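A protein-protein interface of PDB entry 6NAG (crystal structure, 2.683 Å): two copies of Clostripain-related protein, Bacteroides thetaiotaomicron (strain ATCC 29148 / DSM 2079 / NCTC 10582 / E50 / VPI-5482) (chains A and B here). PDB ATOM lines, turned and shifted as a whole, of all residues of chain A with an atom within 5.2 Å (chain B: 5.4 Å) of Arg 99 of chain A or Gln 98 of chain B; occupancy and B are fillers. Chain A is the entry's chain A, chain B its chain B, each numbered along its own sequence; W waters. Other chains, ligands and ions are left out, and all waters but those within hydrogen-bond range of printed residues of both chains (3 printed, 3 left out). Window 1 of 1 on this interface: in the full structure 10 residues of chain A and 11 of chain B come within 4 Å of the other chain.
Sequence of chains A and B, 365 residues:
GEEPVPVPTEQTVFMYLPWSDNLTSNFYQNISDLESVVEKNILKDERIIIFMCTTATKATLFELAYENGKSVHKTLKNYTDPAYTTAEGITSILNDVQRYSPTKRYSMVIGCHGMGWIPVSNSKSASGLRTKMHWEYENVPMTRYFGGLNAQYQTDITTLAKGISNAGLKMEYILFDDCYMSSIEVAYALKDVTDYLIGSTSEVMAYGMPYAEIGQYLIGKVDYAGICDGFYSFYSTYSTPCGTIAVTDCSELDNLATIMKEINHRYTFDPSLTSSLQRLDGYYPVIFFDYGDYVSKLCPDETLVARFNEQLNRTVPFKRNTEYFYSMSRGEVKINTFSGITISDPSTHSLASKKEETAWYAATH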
ATOM      1  N   ASN A  95     -14.732  18.041  10.670  1.00  0.00           N
ATOM      2  CA  ASN A  95     -15.767  17.071  11.002  1.00  0.00           C
ATOM      3  C   ASN A  95     -16.013  16.113   9.842  1.00  0.00           C
ATOM      4  O   ASN A  95     -16.205  14.918  10.049  1.00  0.00           O
ATOM      5  CB  ASN A  95     -17.067  17.774  11.393  1.00  0.00           C
ATOM      6  CG  ASN A  95     -17.022  18.345  12.797  1.00  0.00           C
ATOM      7  OD1 ASN A  95     -16.238  17.899  13.634  1.00  0.00           O
ATOM      8  ND2 ASN A  95     -17.870  19.330  13.064  1.00  0.00           N
ATOM      9  N   ASP A  96     -16.002  16.644   8.623  1.00  0.00           N
ATOM     10  CA  ASP A  96     -16.144  15.821   7.426  1.00  0.00           C
ATOM     11  C   ASP A  96     -15.001  14.819   7.320  1.00  0.00           C
ATOM     12  O   ASP A  96     -15.202  13.674   6.920  1.00  0.00           O
ATOM     13  CB  ASP A  96     -16.195  16.691   6.168  1.00  0.00           C
ATOM     14  CG  ASP A  96     -17.455  17.529   6.086  1.00  0.00           C
ATOM     15  OD1 ASP A  96     -18.492  17.103   6.636  1.00  0.00           O
ATOM     16  OD2 ASP A  96     -17.409  18.614   5.469  1.00  0.00           O
ATOM     17  N   VAL A  97     -13.801  15.261   7.684  1.00  0.00           N
ATOM     18  CA  VAL A  97     -12.627  14.398   7.686  1.00  0.00           C
ATOM     19  C   VAL A  97     -12.813  13.241   8.664  1.00  0.00           C
ATOM     20  O   VAL A  97     -12.477  12.097   8.361  1.00  0.00           O
ATOM     21  CB  VAL A  97     -11.350  15.184   8.050  1.00  0.00           C
ATOM     22  CG1 VAL A  97     -10.154  14.252   8.158  1.00  0.00           C
ATOM     23  CG2 VAL A  97     -11.091  16.276   7.025  1.00  0.00           C
ATOM     24  N   GLN A  98     -13.365  13.549   9.833  1.00  0.00           N
ATOM     25  CA  GLN A  98     -13.601  12.546  10.864  1.00  0.00           C
ATOM     26  C   GLN A  98     -14.638  11.511  10.436  1.00  0.00           C
ATOM     27  O   GLN A  98     -14.504  10.328  10.742  1.00  0.00           O
ATOM     28  CB  GLN A  98     -14.048  13.215  12.165  1.00  0.00           C
ATOM     29  CG  GLN A  98     -12.990  14.089  12.812  1.00  0.00           C
ATOM     30  CD  GLN A  98     -13.521  14.848  14.011  1.00  0.00           C
ATOM     31  OE1 GLN A  98     -13.880  14.254  15.026  1.00  0.00           O
ATOM     32  NE2 GLN A  98     -13.575  16.170  13.898  1.00  0.00           N
ATOM     33  N   ARG A  99     -15.672  11.958   9.730  1.00  0.00           N
ATOM     34  CA  ARG A  99     -16.749  11.066   9.315  1.00  0.00           C
ATOM     35  C   ARG A  99     -16.326  10.179   8.147  1.00  0.00           C
ATOM     36  O   ARG A  99     -16.613   8.983   8.135  1.00  0.00           O
ATOM     37  CB  ARG A  99     -17.999  11.864   8.938  1.00  0.00           C
ATOM     38  CG  ARG A  99     -18.492  12.808  10.022  1.00  0.00           C
ATOM     39  CD  ARG A  99     -18.689  12.097  11.352  1.00  0.00           C
ATOM     40  NE  ARG A  99     -19.088  13.026  12.405  1.00  0.00           N
ATOM     41  CZ  ARG A  99     -18.297  13.413  13.403  1.00  0.00           C
ATOM     42  NH1 ARG A  99     -18.744  14.264  14.316  1.00  0.00           N
ATOM     43  NH2 ARG A  99     -17.061  12.944  13.490  1.00  0.00           N
ATOM     44  N   TYR A 100     -15.647  10.768   7.168  1.00  0.00           N
ATOM     45  CA  TYR A 100     -15.193  10.013   6.006  1.00  0.00           C
ATOM     46  C   TYR A 100     -13.957   9.181   6.331  1.00  0.00           C
ATOM     47  O   TYR A 100     -13.714   8.147   5.709  1.00  0.00           O
ATOM     48  CB  TYR A 100     -14.905  10.950   4.830  1.00  0.00           C
ATOM     49  CG  TYR A 100     -16.149  11.452   4.133  1.00  0.00           C
ATOM     50  CD1 TYR A 100     -16.893  10.615   3.314  1.00  0.00           C
ATOM     51  CD2 TYR A 100     -16.578  12.763   4.291  1.00  0.00           C
ATOM     52  CE1 TYR A 100     -18.031  11.066   2.675  1.00  0.00           C
ATOM     53  CE2 TYR A 100     -17.715  13.225   3.655  1.00  0.00           C
ATOM     54  CZ  TYR A 100     -18.437  12.372   2.847  1.00  0.00           C
ATOM     55  OH  TYR A 100     -19.568  12.826   2.212  1.00  0.00           O
ATOM     56  N   SER A 101     -13.179   9.635   7.307  1.00  0.00           N
ATOM     57  CA  SER A 101     -11.987   8.907   7.726  1.00  0.00           C
ATOM     58  C   SER A 101     -11.895   8.809   9.247  1.00  0.00           C
ATOM     59  O   SER A 101     -11.131   9.540   9.874  1.00  0.00           O
ATOM     60  CB  SER A 101     -10.729   9.575   7.168  1.00  0.00           C
ATOM     61  OG  SER A 101      -9.564   8.849   7.522  1.00  0.00           O
ATOM     62  N   PRO A 102     -12.682   7.900   9.845  1.00  0.00           N
ATOM     63  CA  PRO A 102     -12.647   7.688  11.296  1.00  0.00           C
ATOM     64  C   PRO A 102     -11.403   6.922  11.744  1.00  0.00           C
ATOM     65  O   PRO A 102     -11.301   5.716  11.517  1.00  0.00           O
ATOM     66  CB  PRO A 102     -13.918   6.877  11.560  1.00  0.00           C
ATOM     67  CG  PRO A 102     -14.167   6.153  10.286  1.00  0.00           C
ATOM     68  CD  PRO A 102     -13.701   7.063   9.186  1.00  0.00           C
ATOM     69  N   ALA A 167     -13.856  20.976  16.782  1.00  0.00           N
ATOM     70  CA  ALA A 167     -14.042  19.732  16.049  1.00  0.00           C
ATOM     71  C   ALA A 167     -13.773  18.543  16.964  1.00  0.00           C
ATOM     72  O   ALA A 167     -13.979  17.391  16.583  1.00  0.00           O
ATOM     73  CB  ALA A 167     -13.136  19.688  14.831  1.00  0.00           C
ATOM     74  N   PRO B   8     -20.008   7.081   5.750  1.00  0.00           N
ATOM     75  CA  PRO B   8     -20.923   7.540   6.805  1.00  0.00           C
ATOM     76  C   PRO B   8     -22.391   7.575   6.382  1.00  0.00           C
ATOM     77  O   PRO B   8     -22.695   7.640   5.190  1.00  0.00           O
ATOM     78  CB  PRO B   8     -20.420   8.958   7.114  1.00  0.00           C
ATOM     79  CG  PRO B   8     -19.600   9.352   5.930  1.00  0.00           C
ATOM     80  CD  PRO B   8     -18.966   8.083   5.467  1.00  0.00           C
ATOM     81  N   ILE B  93     -15.539   8.513  25.476  1.00  0.00           N
ATOM     82  CA  ILE B  93     -16.612   7.600  25.099  1.00  0.00           C
ATOM     83  C   ILE B  93     -17.343   8.107  23.860  1.00  0.00           C
ATOM     84  O   ILE B  93     -17.618   7.345  22.934  1.00  0.00           O
ATOM     85  CB  ILE B  93     -17.619   7.408  26.252  1.00  0.00           C
ATOM     86  CG1 ILE B  93     -16.936   6.733  27.443  1.00  0.00           C
ATOM     87  CG2 ILE B  93     -18.811   6.582  25.795  1.00  0.00           C
ATOM     88  CD1 ILE B  93     -17.793   6.676  28.687  1.00  0.00           C
ATOM     89  N   LEU B  94     -17.645   9.402  23.844  1.00  0.00           N
ATOM     90  CA  LEU B  94     -18.320  10.016  22.707  1.00  0.00           C
ATOM     91  C   LEU B  94     -17.442   9.992  21.461  1.00  0.00           C
ATOM     92  O   LEU B  94     -17.946   9.936  20.340  1.00  0.00           O
ATOM     93  CB  LEU B  94     -18.730  11.451  23.035  1.00  0.00           C
ATOM     94  CG  LEU B  94     -19.930  11.592  23.973  1.00  0.00           C
ATOM     95  CD1 LEU B  94     -20.185  13.051  24.296  1.00  0.00           C
ATOM     96  CD2 LEU B  94     -21.164  10.952  23.357  1.00  0.00           C
ATOM     97  N   ASN B  95     -16.128  10.034  21.661  1.00  0.00           N
ATOM     98  CA  ASN B  95     -15.191   9.907  20.553  1.00  0.00           C
ATOM     99  C   ASN B  95     -15.234   8.503  19.961  1.00  0.00           C
ATOM    100  O   ASN B  95     -15.122   8.331  18.749  1.00  0.00           O
ATOM    101  CB  ASN B  95     -13.768  10.248  20.998  1.00  0.00           C
ATOM    102  CG  ASN B  95     -13.522  11.744  21.068  1.00  0.00           C
ATOM    103  OD1 ASN B  95     -14.234  12.532  20.446  1.00  0.00           O
ATOM    104  ND2 ASN B  95     -12.504  12.141  21.822  1.00  0.00           N
ATOM    105  N   ASP B  96     -15.400   7.504  20.824  1.00  0.00           N
ATOM    106  CA  ASP B  96     -15.541   6.122  20.379  1.00  0.00           C
ATOM    107  C   ASP B  96     -16.790   5.961  19.524  1.00  0.00           C
ATOM    108  O   ASP B  96     -16.787   5.232  18.533  1.00  0.00           O
ATOM    109  CB  ASP B  96     -15.596   5.167  21.574  1.00  0.00           C
ATOM    110  CG  ASP B  96     -14.284   5.093  22.327  1.00  0.00           C
ATOM    111  OD1 ASP B  96     -13.228   5.370  21.719  1.00  0.00           O
ATOM    112  OD2 ASP B  96     -14.307   4.753  23.529  1.00  0.00           O
ATOM    113  N   VAL B  97     -17.859   6.647  19.916  1.00  0.00           N
ATOM    114  CA  VAL B  97     -19.112   6.610  19.174  1.00  0.00           C
ATOM    115  C   VAL B  97     -18.928   7.200  17.779  1.00  0.00           C
ATOM    116  O   VAL B  97     -19.438   6.664  16.797  1.00  0.00           O
ATOM    117  CB  VAL B  97     -20.227   7.374  19.918  1.00  0.00           C
ATOM    118  CG1 VAL B  97     -21.513   7.373  19.107  1.00  0.00           C
ATOM    119  CG2 VAL B  97     -20.458   6.766  21.291  1.00  0.00           C
ATOM    120  N   GLN B  98     -18.184   8.299  17.700  1.00  0.00           N
ATOM    121  CA  GLN B  98     -17.915   8.962  16.427  1.00  0.00           C
ATOM    122  C   GLN B  98     -17.097   8.084  15.486  1.00  0.00           C
ATOM    123  O   GLN B  98     -17.340   8.059  14.282  1.00  0.00           O
ATOM    124  CB  GLN B  98     -17.180  10.284  16.659  1.00  0.00           C
ATOM    125  CG  GLN B  98     -17.991  11.336  17.386  1.00  0.00           C
ATOM    126  CD  GLN B  98     -17.185  12.585  17.674  1.00  0.00           C
ATOM    127  OE1 GLN B  98     -16.747  13.278  16.757  1.00  0.00           O
ATOM    128  NE2 GLN B  98     -16.983  12.879  18.952  1.00  0.00           N
ATOM    129  N   ARG B  99     -16.123   7.370  16.040  1.00  0.00           N
ATOM    130  CA  ARG B  99     -15.232   6.546  15.231  1.00  0.00           C
ATOM    131  C   ARG B  99     -15.914   5.265  14.759  1.00  0.00           C
ATOM    132  O   ARG B  99     -15.809   4.894  13.591  1.00  0.00           O
ATOM    133  CB  ARG B  99     -13.962   6.204  16.015  1.00  0.00           C
ATOM    134  CG  ARG B  99     -13.153   7.412  16.463  1.00  0.00           C
ATOM    135  CD  ARG B  99     -12.662   8.235  15.283  1.00  0.00           C
ATOM    136  NE  ARG B  99     -13.411   9.478  15.125  1.00  0.00           N
ATOM    137  CZ  ARG B  99     -13.066  10.635  15.681  1.00  0.00           C
ATOM    138  NH1 ARG B  99     -13.807  11.717  15.482  1.00  0.00           N
ATOM    139  NH2 ARG B  99     -11.980  10.713  16.438  1.00  0.00           N
ATOM    140  N   TYR B 100     -16.611   4.590  15.668  1.00  0.00           N
ATOM    141  CA  TYR B 100     -17.293   3.345  15.330  1.00  0.00           C
ATOM    142  C   TYR B 100     -18.567   3.601  14.532  1.00  0.00           C
ATOM    143  O   TYR B 100     -19.002   2.751  13.756  1.00  0.00           O
ATOM    144  CB  TYR B 100     -17.622   2.547  16.595  1.00  0.00           C
ATOM    145  CG  TYR B 100     -16.428   1.856  17.214  1.00  0.00           C
ATOM    146  CD1 TYR B 100     -15.825   0.776  16.584  1.00  0.00           C
ATOM    147  CD2 TYR B 100     -15.911   2.275  18.432  1.00  0.00           C
ATOM    148  CE1 TYR B 100     -14.735   0.139  17.145  1.00  0.00           C
ATOM    149  CE2 TYR B 100     -14.821   1.644  19.002  1.00  0.00           C
ATOM    150  CZ  TYR B 100     -14.238   0.576  18.353  1.00  0.00           C
ATOM    151  OH  TYR B 100     -13.153  -0.057  18.916  1.00  0.00           O
ATOM    152  N   SER B 101     -19.162   4.773  14.724  1.00  0.00           N
ATOM    153  CA  SER B 101     -20.392   5.127  14.024  1.00  0.00           C
ATOM    154  C   SER B 101     -20.334   6.541  13.451  1.00  0.00           C
ATOM    155  O   SER B 101     -20.916   7.467  14.014  1.00  0.00           O
ATOM    156  CB  SER B 101     -21.591   4.993  14.963  1.00  0.00           C
ATOM    157  OG  SER B 101     -22.798   5.336  14.306  1.00  0.00           O
ATOM    158  N   PRO B 102     -19.627   6.711  12.323  1.00  0.00           N
ATOM    159  CA  PRO B 102     -19.515   8.016  11.664  1.00  0.00           C
ATOM    160  C   PRO B 102     -20.816   8.425  10.980  1.00  0.00           C
ATOM    161  O   PRO B 102     -21.215   7.789  10.008  1.00  0.00           O
ATOM    162  CB  PRO B 102     -18.406   7.798  10.624  1.00  0.00           C
ATOM    163  CG  PRO B 102     -17.753   6.499  10.995  1.00  0.00           C
ATOM    164  CD  PRO B 102     -18.824   5.688  11.637  1.00  0.00           C
ATOM    165  N   THR B 103     -21.468   9.466  11.489  1.00  0.00           N
ATOM    166  CA  THR B 103     -22.705   9.961  10.892  1.00  0.00           C
ATOM    167  C   THR B 103     -22.749  11.484  10.888  1.00  0.00           C
ATOM    168  O   THR B 103     -21.912  12.140  11.505  1.00  0.00           O
ATOM    169  CB  THR B 103     -23.951   9.430  11.629  1.00  0.00           C
ATOM    170  OG1 THR B 103     -23.794   9.623  13.040  1.00  0.00           O
ATOM    171  CG2 THR B 103     -24.158   7.952  11.345  1.00  0.00           C
ATOM    172  N   LYS B 104     -23.732  12.040  10.189  1.00  0.00           N
ATOM    173  CA  LYS B 104     -23.902  13.487  10.131  1.00  0.00           C
ATOM    174  C   LYS B 104     -24.524  14.012  11.419  1.00  0.00           C
ATOM    175  O   LYS B 104     -24.068  15.009  11.979  1.00  0.00           O
ATOM    176  CB  LYS B 104     -24.767  13.878   8.931  1.00  0.00           C
ATOM    177  CG  LYS B 104     -24.163  13.509   7.587  1.00  0.00           C
ATOM    178  CD  LYS B 104     -25.078  13.901   6.439  1.00  0.00           C
ATOM    179  CE  LYS B 104     -24.426  13.620   5.093  1.00  0.00           C
ATOM    180  NZ  LYS B 104     -23.941  12.215   4.986  1.00  0.00           N
ATOM    181  N   TYR B 106     -26.025  13.330  15.465  1.00  0.00           N
ATOM    182  CA  TYR B 106     -25.869  12.527  16.668  1.00  0.00           C
ATOM    183  C   TYR B 106     -26.916  12.912  17.704  1.00  0.00           C
ATOM    184  O   TYR B 106     -27.227  14.088  17.879  1.00  0.00           O
ATOM    185  CB  TYR B 106     -24.463  12.689  17.253  1.00  0.00           C
ATOM    186  CG  TYR B 106     -23.383  11.995  16.455  1.00  0.00           C
ATOM    187  CD1 TYR B 106     -22.732  12.648  15.417  1.00  0.00           C
ATOM    188  CD2 TYR B 106     -23.015  10.687  16.740  1.00  0.00           C
ATOM    189  CE1 TYR B 106     -21.746  12.016  14.684  1.00  0.00           C
ATOM    190  CE2 TYR B 106     -22.031  10.048  16.013  1.00  0.00           C
ATOM    191  CZ  TYR B 106     -21.400  10.716  14.986  1.00  0.00           C
ATOM    192  OH  TYR B 106     -20.418  10.082  14.260  1.00  0.00           O
ATOM    193  N   ALA B 167     -15.814  16.727  22.594  1.00  0.00           N
ATOM    194  CA  ALA B 167     -15.865  15.654  21.611  1.00  0.00           C
ATOM    195  C   ALA B 167     -16.209  16.220  20.237  1.00  0.00           C
ATOM    196  O   ALA B 167     -16.260  15.492  19.248  1.00  0.00           O
ATOM    197  CB  ALA B 167     -16.874  14.597  22.023  1.00  0.00           C
ATOM    198  N   GLY B 168     -16.444  17.527  20.189  1.00  0.00           N
ATOM    199  CA  GLY B 168     -16.765  18.206  18.948  1.00  0.00           C
ATOM    200  C   GLY B 168     -18.150  17.870  18.433  1.00  0.00           C
ATOM    201  O   GLY B 168     -18.376  17.818  17.224  1.00  0.00           O
ATOM    202  N   LEU B 169     -19.083  17.646  19.352  1.00  0.00           N
ATOM    203  CA  LEU B 169     -20.440  17.271  18.979  1.00  0.00           C
ATOM    204  C   LEU B 169     -21.481  18.264  19.476  1.00  0.00           C
ATOM    205  O   LEU B 169     -21.304  18.906  20.511  1.00  0.00           O
ATOM    206  CB  LEU B 169     -20.777  15.877  19.518  1.00  0.00           C
ATOM    207  CG  LEU B 169     -19.991  14.687  18.970  1.00  0.00           C
ATOM    208  CD1 LEU B 169     -20.483  13.396  19.602  1.00  0.00           C
ATOM    209  CD2 LEU B 169     -20.100  14.623  17.455  1.00  0.00           C
HETATM  210  O   HOH W   1     -18.217  20.418  16.022  1.00  0.00           O
HETATM  211  O   HOH W   2     -21.022  15.204  12.106  1.00  0.00           O
HETATM  212  O   HOH W   3     -15.629  10.009  13.279  1.00  0.00           O
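NE2 of Gln 98 of chain A lies within hydrogen-bond range of OD1 of Asn 95 of chain A (3.2 Å). NE2 of Gln 98 of chain A lies within hydrogen-bond range of O of Ala 167 of chain A, 3.0 Å away. The backbone carbonyl oxygen of Leu 94 of chain B lies close to the side-chain amide nitrogen of Gln 98 of chain B, at 3.4 Å. The side-chain amide oxygen (OD1) of Asn 95 of chain B lies within hydrogen-bond range of the side-chain amide nitrogen (NE2) of Gln 98 of chain B (3.1 Å). NE2 of Gln 98 of chain B is in hydrogen-bond range of O of Ala 167 of chain B. The backbone NH (N) of Thr 103 of chain B sits at hydrogen-bond distance from the side-chain hydroxyl (OH) of Tyr 106 of chain B.
O of Arg 99 of chain A touches CD of Pro 8 of chain B, at 3.7 Å. Pro 102 of chain B touches Arg 99 of chain A. Tyr 106 of chain B touches Arg 99 of chain A. Arg 99 of chain A touches Leu 169 of chain B (NH1 to CD2, 3.4 Å). Tyr 100 of chain A touches Pro 8 of chain B (CD1 to CD, 3.9 Å). CB of Pro 102 of chain A touches O of Arg 99 of chain B, 3.4 Å away. Pro 102 of chain A touches Pro 102 of chain B (CG to CG, 3.7 Å). Ala 167 of chain B touches Ala 167 of chain A (O to O, 3.99 Å). Ala 167 of chain A touches Gly 168 of chain B.
Water W3 lies within hydrogen-bond range of O of Gln 98 of chain B (2.8 Å), O of Gln 98 of chain A (2.8 Å), NE of Arg 99 of chain B (2.9 Å) and NH2 of Arg 99 of chain A (3.3 Å). Water W1 lies within hydrogen-bond range of O of Gly 168 of chain B (2.9 Å) and ND2 of Asn 95 of chain A (3.2 Å). Water W2 lies within hydrogen-bond range of NE of Arg 99 of chain A (2.9 Å), O of Lys 104 of chain B (3.1 Å) and O of Thr 103 of chain B (3.2 Å).
The side-chain amide oxygen of Gln 98 of chain A lies close to the side-chain amide oxygen of Gln 98 of chain B (3.5 Å). The side-chain amide oxygen of Gln 98 of chain A sits at hydrogen-bond distance from the guanidinium group of Arg 99 of chain B. OE1 of Gln 98 of chain B lies within hydrogen-bond range of NH2 of Arg 99 of chain A, 3.3 Å away. The guanidinium group (NE) of Arg 99 of chain A sits at hydrogen-bond distance from the backbone carbonyl oxygen (O) of Thr 103 of chain B (3.1 Å).
Gln 98 of chain B touches its own counterpart, Gln 98 of chain A. Arg 99 of chain A touches Pro 102 of chain B, and with the chains exchanged Pro 102 of chain A touches Arg 99 of chain B. Pro 102 of chain B touches its own counterpart, Pro 102 of chain A. Ala 167 of chain B touches its own counterpart, Ala 167 of chain A. Of the 13 pairs that touch across the chains among the printed residues, 7 have their exchanged pair printed and touching as well.
Of the 9 printed residues of chain A, 5 touch a printed residue of chain B. Printed residues of chain A that touch a printed residue of chain B: Gln 98, Arg 99, Tyr 100, Pro 102 and Ala 167. Hydrophobic or aromatic side chains of chain B that line the printed part of chain A: Pro 8, Pro 102, Tyr 106 and Leu 169. Among the printed residues, 13 pairs touch across the chains. Among the printed residues, no Asp or Glu carboxylate lies within 4 Å of a Lys or Arg side-chain nitrogen of the other chain.
Printed residues of chain B within 4 Å of Arg 99 of chain A: Pro 8 (3.7 Å), Gln 98 (3.3 Å), Pro 102 (3.3 Å), Thr 103 (3.1 Å), Tyr 106 (3.6 Å) and Leu 169 (3.4 Å). Gln 98 of chain B touches just these residues of chain A: Gln 98 and Arg 99. Of the printed residues of chain A, Ala 167 of chain B touches Ala 167 (3.99 Å). Of the printed residues of chain A, Pro 8 of chain B touches Arg 99 (3.7 Å) and Tyr 100 (3.9 Å). The nearest printed residue of chain B that does not touch Arg 99 of chain A is Arg 99 of chain B (4.01 Å). The nearest residue of chain A that does not touch Gln 98 of chain B is Pro 102 of chain A (4.5 Å).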
